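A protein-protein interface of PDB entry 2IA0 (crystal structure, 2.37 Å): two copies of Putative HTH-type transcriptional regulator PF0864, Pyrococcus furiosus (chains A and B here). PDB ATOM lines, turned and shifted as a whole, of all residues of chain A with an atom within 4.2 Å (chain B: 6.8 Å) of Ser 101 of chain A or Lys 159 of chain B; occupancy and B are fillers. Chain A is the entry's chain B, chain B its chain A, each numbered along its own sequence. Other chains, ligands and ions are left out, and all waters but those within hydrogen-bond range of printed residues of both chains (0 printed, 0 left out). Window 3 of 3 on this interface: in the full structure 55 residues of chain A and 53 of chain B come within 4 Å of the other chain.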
ATOM      1  N   ILE A  97     -27.006  16.608  13.004  1.00  0.00           N
ATOM      2  CA  ILE A  97     -26.320  17.745  12.399  1.00  0.00           C
ATOM      3  C   ILE A  97     -25.612  17.381  11.095  1.00  0.00           C
ATOM      4  O   ILE A  97     -25.719  18.118  10.122  1.00  0.00           O
ATOM      5  CB  ILE A  97     -25.369  18.454  13.384  1.00  0.00           C
ATOM      6  CG1 ILE A  97     -26.190  19.225  14.409  1.00  0.00           C
ATOM      7  CG2 ILE A  97     -24.429  19.436  12.648  1.00  0.00           C
ATOM      8  CD1 ILE A  97     -25.663  19.034  15.776  1.00  0.00           C
ATOM      9  N   SER A  98     -24.922  16.241  11.065  1.00  0.00           N
ATOM     10  CA  SER A  98     -24.357  15.711   9.799  1.00  0.00           C
ATOM     11  C   SER A  98     -25.409  15.529   8.665  1.00  0.00           C
ATOM     12  O   SER A  98     -25.183  15.887   7.504  1.00  0.00           O
ATOM     13  CB  SER A  98     -23.635  14.395  10.073  1.00  0.00           C
ATOM     14  OG  SER A  98     -22.674  14.142   9.081  1.00  0.00           O
ATOM     15  N   TYR A  99     -26.566  14.987   9.017  1.00  0.00           N
ATOM     16  CA  TYR A  99     -27.667  14.835   8.077  1.00  0.00           C
ATOM     17  C   TYR A  99     -28.245  16.173   7.573  1.00  0.00           C
ATOM     18  O   TYR A  99     -28.412  16.341   6.368  1.00  0.00           O
ATOM     19  CB  TYR A  99     -28.776  13.935   8.664  1.00  0.00           C
ATOM     20  CG  TYR A  99     -30.133  14.167   8.034  1.00  0.00           C
ATOM     21  CD1 TYR A  99     -30.378  13.793   6.718  1.00  0.00           C
ATOM     22  CD2 TYR A  99     -31.169  14.760   8.755  1.00  0.00           C
ATOM     23  CE1 TYR A  99     -31.607  14.016   6.120  1.00  0.00           C
ATOM     24  CE2 TYR A  99     -32.424  14.983   8.164  1.00  0.00           C
ATOM     25  CZ  TYR A  99     -32.623  14.611   6.837  1.00  0.00           C
ATOM     26  OH  TYR A  99     -33.844  14.815   6.217  1.00  0.00           O
ATOM     27  N   ILE A 100     -28.552  17.103   8.482  1.00  0.00           N
ATOM     28  CA  ILE A 100     -29.113  18.410   8.109  1.00  0.00           C
ATOM     29  C   ILE A 100     -28.143  19.164   7.251  1.00  0.00           C
ATOM     30  O   ILE A 100     -28.522  19.783   6.266  1.00  0.00           O
ATOM     31  CB  ILE A 100     -29.427  19.326   9.333  1.00  0.00           C
ATOM     32  CG1 ILE A 100     -30.562  18.757  10.181  1.00  0.00           C
ATOM     33  CG2 ILE A 100     -29.794  20.760   8.877  1.00  0.00           C
ATOM     34  CD1 ILE A 100     -30.677  19.486  11.568  1.00  0.00           C
ATOM     35  N   SER A 101     -26.877  19.118   7.629  1.00  0.00           N
ATOM     36  CA  SER A 101     -25.909  19.903   6.919  1.00  0.00           C
ATOM     37  C   SER A 101     -25.583  19.327   5.521  1.00  0.00           C
ATOM     38  O   SER A 101     -25.343  20.104   4.595  1.00  0.00           O
ATOM     39  CB  SER A 101     -24.697  20.184   7.794  1.00  0.00           C
ATOM     40  OG  SER A 101     -23.811  19.094   7.792  1.00  0.00           O
ATOM     41  N   SER A 102     -25.625  17.998   5.329  1.00  0.00           N
ATOM     42  CA  SER A 102     -25.451  17.469   3.949  1.00  0.00           C
ATOM     43  C   SER A 102     -26.658  17.725   3.080  1.00  0.00           C
ATOM     44  O   SER A 102     -26.541  17.888   1.865  1.00  0.00           O
ATOM     45  CB  SER A 102     -25.017  15.989   3.872  1.00  0.00           C
ATOM     46  OG  SER A 102     -25.595  15.213   4.887  1.00  0.00           O
ATOM     47  N   THR A 103     -27.818  17.767   3.710  1.00  0.00           N
ATOM     48  CA  THR A 103     -29.069  18.075   3.027  1.00  0.00           C
ATOM     49  C   THR A 103     -29.111  19.520   2.519  1.00  0.00           C
ATOM     50  O   THR A 103     -29.543  19.780   1.402  1.00  0.00           O
ATOM     51  CB  THR A 103     -30.243  17.839   3.979  1.00  0.00           C
ATOM     52  OG1 THR A 103     -30.257  16.457   4.337  1.00  0.00           O
ATOM     53  CG2 THR A 103     -31.550  18.227   3.337  1.00  0.00           C
ATOM     54  N   LEU A 104     -28.690  20.444   3.375  1.00  0.00           N
ATOM     55  CA  LEU A 104     -28.507  21.850   3.015  1.00  0.00           C
ATOM     56  C   LEU A 104     -27.397  22.079   2.001  1.00  0.00           C
ATOM     57  O   LEU A 104     -27.536  22.909   1.120  1.00  0.00           O
ATOM     58  CB  LEU A 104     -28.252  22.684   4.266  1.00  0.00           C
ATOM     59  CG  LEU A 104     -29.442  22.729   5.232  1.00  0.00           C
ATOM     60  CD1 LEU A 104     -29.206  23.792   6.289  1.00  0.00           C
ATOM     61  CD2 LEU A 104     -30.770  22.954   4.497  1.00  0.00           C
ATOM     62  N   SER A 105     -26.299  21.346   2.122  1.00  0.00           N
ATOM     63  CA  SER A 105     -25.208  21.454   1.153  1.00  0.00           C
ATOM     64  C   SER A 105     -25.571  21.072  -0.298  1.00  0.00           C
ATOM     65  O   SER A 105     -25.046  21.644  -1.254  1.00  0.00           O
ATOM     66  CB  SER A 105     -23.998  20.692   1.658  1.00  0.00           C
ATOM     67  OG  SER A 105     -23.531  21.302   2.854  1.00  0.00           O
ATOM     68  N   VAL A 113     -22.109  26.343   4.429  1.00  0.00           N
ATOM     69  CA  VAL A 113     -22.661  25.552   5.553  1.00  0.00           C
ATOM     70  C   VAL A 113     -21.525  25.204   6.535  1.00  0.00           C
ATOM     71  O   VAL A 113     -20.427  24.775   6.135  1.00  0.00           O
ATOM     72  CB  VAL A 113     -23.451  24.262   5.108  1.00  0.00           C
ATOM     73  CG1 VAL A 113     -24.172  23.596   6.312  1.00  0.00           C
ATOM     74  CG2 VAL A 113     -24.500  24.576   4.025  1.00  0.00           C
ATOM     75  N   ALA A 114     -21.784  25.442   7.816  1.00  0.00           N
ATOM     76  CA  ALA A 114     -20.814  25.238   8.873  1.00  0.00           C
ATOM     77  C   ALA A 114     -21.493  24.712  10.130  1.00  0.00           C
ATOM     78  O   ALA A 114     -22.646  25.088  10.442  1.00  0.00           O
ATOM     79  CB  ALA A 114     -20.151  26.547   9.200  1.00  0.00           C
ATOM     80  N   ILE A 121     -26.023  24.880  13.256  1.00  0.00           N
ATOM     81  CA  ILE A 121     -25.640  25.043  11.864  1.00  0.00           C
ATOM     82  C   ILE A 121     -25.758  26.508  11.437  1.00  0.00           C
ATOM     83  O   ILE A 121     -26.741  27.166  11.734  1.00  0.00           O
ATOM     84  CB  ILE A 121     -26.459  24.106  10.929  1.00  0.00           C
ATOM     85  CG1 ILE A 121     -26.093  22.659  11.238  1.00  0.00           C
ATOM     86  CG2 ILE A 121     -26.176  24.389   9.452  1.00  0.00           C
ATOM     87  CD1 ILE A 121     -26.856  21.646  10.433  1.00  0.00           C
ATOM     88  N   GLU B 157     -16.648  23.286  12.205  1.00  0.00           N
ATOM     89  CA  GLU B 157     -16.345  22.537  11.011  1.00  0.00           C
ATOM     90  C   GLU B 157     -17.081  23.165   9.833  1.00  0.00           C
ATOM     91  O   GLU B 157     -18.285  23.341   9.895  1.00  0.00           O
ATOM     92  CB  GLU B 157     -16.813  21.096  11.214  1.00  0.00           C
ATOM     93  CG  GLU B 157     -16.424  20.158  10.113  1.00  0.00           C
ATOM     94  CD  GLU B 157     -16.989  18.767  10.322  1.00  0.00           C
ATOM     95  OE1 GLU B 157     -16.772  17.914   9.432  1.00  0.00           O
ATOM     96  OE2 GLU B 157     -17.658  18.526  11.361  1.00  0.00           O
ATOM     97  N   ILE B 158     -16.372  23.503   8.765  1.00  0.00           N
ATOM     98  CA  ILE B 158     -17.055  23.961   7.556  1.00  0.00           C
ATOM     99  C   ILE B 158     -17.451  22.783   6.657  1.00  0.00           C
ATOM    100  O   ILE B 158     -16.614  22.011   6.255  1.00  0.00           O
ATOM    101  CB  ILE B 158     -16.235  25.000   6.755  1.00  0.00           C
ATOM    102  CG1 ILE B 158     -15.893  26.211   7.649  1.00  0.00           C
ATOM    103  CG2 ILE B 158     -16.995  25.402   5.497  1.00  0.00           C
ATOM    104  CD1 ILE B 158     -15.162  27.378   6.944  1.00  0.00           C
ATOM    105  N   LYS B 159     -18.728  22.669   6.325  1.00  0.00           N
ATOM    106  CA  LYS B 159     -19.203  21.545   5.516  1.00  0.00           C
ATOM    107  C   LYS B 159     -19.282  21.870   4.008  1.00  0.00           C
ATOM    108  O   LYS B 159     -18.922  21.031   3.196  1.00  0.00           O
ATOM    109  CB  LYS B 159     -20.529  20.996   6.084  1.00  0.00           C
ATOM    110  CG  LYS B 159     -20.447  20.531   7.606  1.00  0.00           C
ATOM    111  CD  LYS B 159     -20.000  19.042   7.752  1.00  0.00           C
ATOM    112  CE  LYS B 159     -20.062  18.484   9.222  1.00  0.00           C
ATOM    113  NZ  LYS B 159     -21.400  18.478   9.978  1.00  0.00           N
ATOM    114  N   LYS B 160     -19.763  23.067   3.658  1.00  0.00           N
ATOM    115  CA  LYS B 160     -19.758  23.616   2.293  1.00  0.00           C
ATOM    116  C   LYS B 160     -19.110  24.989   2.376  1.00  0.00           C
ATOM    117  O   LYS B 160     -19.359  25.725   3.325  1.00  0.00           O
ATOM    118  CB  LYS B 160     -21.174  23.781   1.734  1.00  0.00           C
ATOM    119  CG  LYS B 160     -21.239  23.945   0.208  1.00  0.00           C
ATOM    120  CD  LYS B 160     -22.612  24.472  -0.273  1.00  0.00           C
ATOM    121  CE  LYS B 160     -22.751  24.300  -1.814  1.00  0.00           C
ATOM    122  NZ  LYS B 160     -24.190  24.160  -2.253  1.00  0.00           N
ATOM    123  N   GLY B 161     -18.263  25.312   1.393  1.00  0.00           N
ATOM    124  CA  GLY B 161     -17.489  26.555   1.348  1.00  0.00           C
ATOM    125  C   GLY B 161     -16.197  26.598   2.170  1.00  0.00           C
ATOM    126  O   GLY B 161     -15.810  27.666   2.635  1.00  0.00           O
ATOM    127  N   GLU B 162     -15.521  25.467   2.372  1.00  0.00           N
ATOM    128  CA  GLU B 162     -14.289  25.475   3.187  1.00  0.00           C
ATOM    129  C   GLU B 162     -13.158  26.407   2.697  1.00  0.00           C
ATOM    130  O   GLU B 162     -12.407  26.974   3.500  1.00  0.00           O
ATOM    131  CB  GLU B 162     -13.763  24.064   3.466  1.00  0.00           C
ATOM    132  CG  GLU B 162     -13.823  23.060   2.317  1.00  0.00           C
ATOM    133  CD  GLU B 162     -13.155  21.723   2.692  1.00  0.00           C
ATOM    134  OE1 GLU B 162     -12.549  21.079   1.800  1.00  0.00           O
ATOM    135  OE2 GLU B 162     -13.231  21.316   3.884  1.00  0.00           O
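OG of Ser 101 of chain A is in hydrogen-bond range of NZ of Lys 159 of chain B (3.3 Å). The backbone NH (N) of Lys 159 of chain B sits at hydrogen-bond distance from the backbone carbonyl oxygen (O) of Val 113 of chain A, 2.7 Å away. The side-chain amino group of Lys 160 of chain B sits at hydrogen-bond distance from the backbone carbonyl oxygen of Ser 105 of chain A. The backbone carbonyl oxygen (O) of Lys 160 of chain B is in hydrogen-bond range of the backbone NH (N) of Val 113 of chain A (3.0 Å).
The side-chain amino group (NZ) of Lys 159 of chain B lies within salt-bridge range of the side-chain carboxylate (OE2) of Glu 157 of chain B, at 3.99 Å. O of Ile 97 of chain A is in hydrogen-bond range of OG of Ser 101 of chain A. The backbone carbonyl oxygen of Ser 98 of chain A sits close to the side-chain hydroxyl of Ser 101 of chain A (3.5 Å). O of Ser 101 of chain A sits at hydrogen-bond distance from OG of Ser 105 of chain A, 2.8 Å away.
Among the printed residues, merely in contact across the chains: Ala 114 of chain A with Glu 157 of chain B and Val 113 of chain A with Ile 158 of chain B.
Ser 101 of chain A touches one residue of chain B. Of the printed residues of chain A, Lys 159 of chain B touches Ser 101 and Val 113. Of the printed residues of chain A, Glu 157 of chain B touches Ala 114. Of the printed residues of chain A, Ile 158 of chain B touches Val 113. Printed residues of chain B within 4 Å of Val 113 of chain A: Ile 158, Lys 159 and Lys 160. Printed residues of chain B within 4 Å of Ala 114 of chain A: Glu 157. Printed residues of chain A within 4 Å of Lys 160 of chain B: Ser 105 and Val 113. Ile 97 of chain A touches none of the printed residues of chain B. Thr 103 of chain A touches none of the printed residues of chain B. The nearest residue of chain B that does not touch Ser 101 of chain A is Lys 160 of chain B (6.3 Å). The nearest residue of chain A that does not touch Lys 159 of chain B is Ser 98 of chain A (4.1 Å).
Of the 12 printed residues of chain A, 4 touch a printed residue of chain B. Hydrophobic or aromatic side chains of chain A within 4 Å of the printed part of chain B: Ala 114. Of the 6 printed residues of chain B, 4 touch a printed residue of chain A. Along chain B the printed residues that touch a printed residue of chain A span positions 157 to 160.
No position is printed for both chains. Of the 6 pairs that touch across the chains among the printed residues, none has its exchanged pair printed and touching as well.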
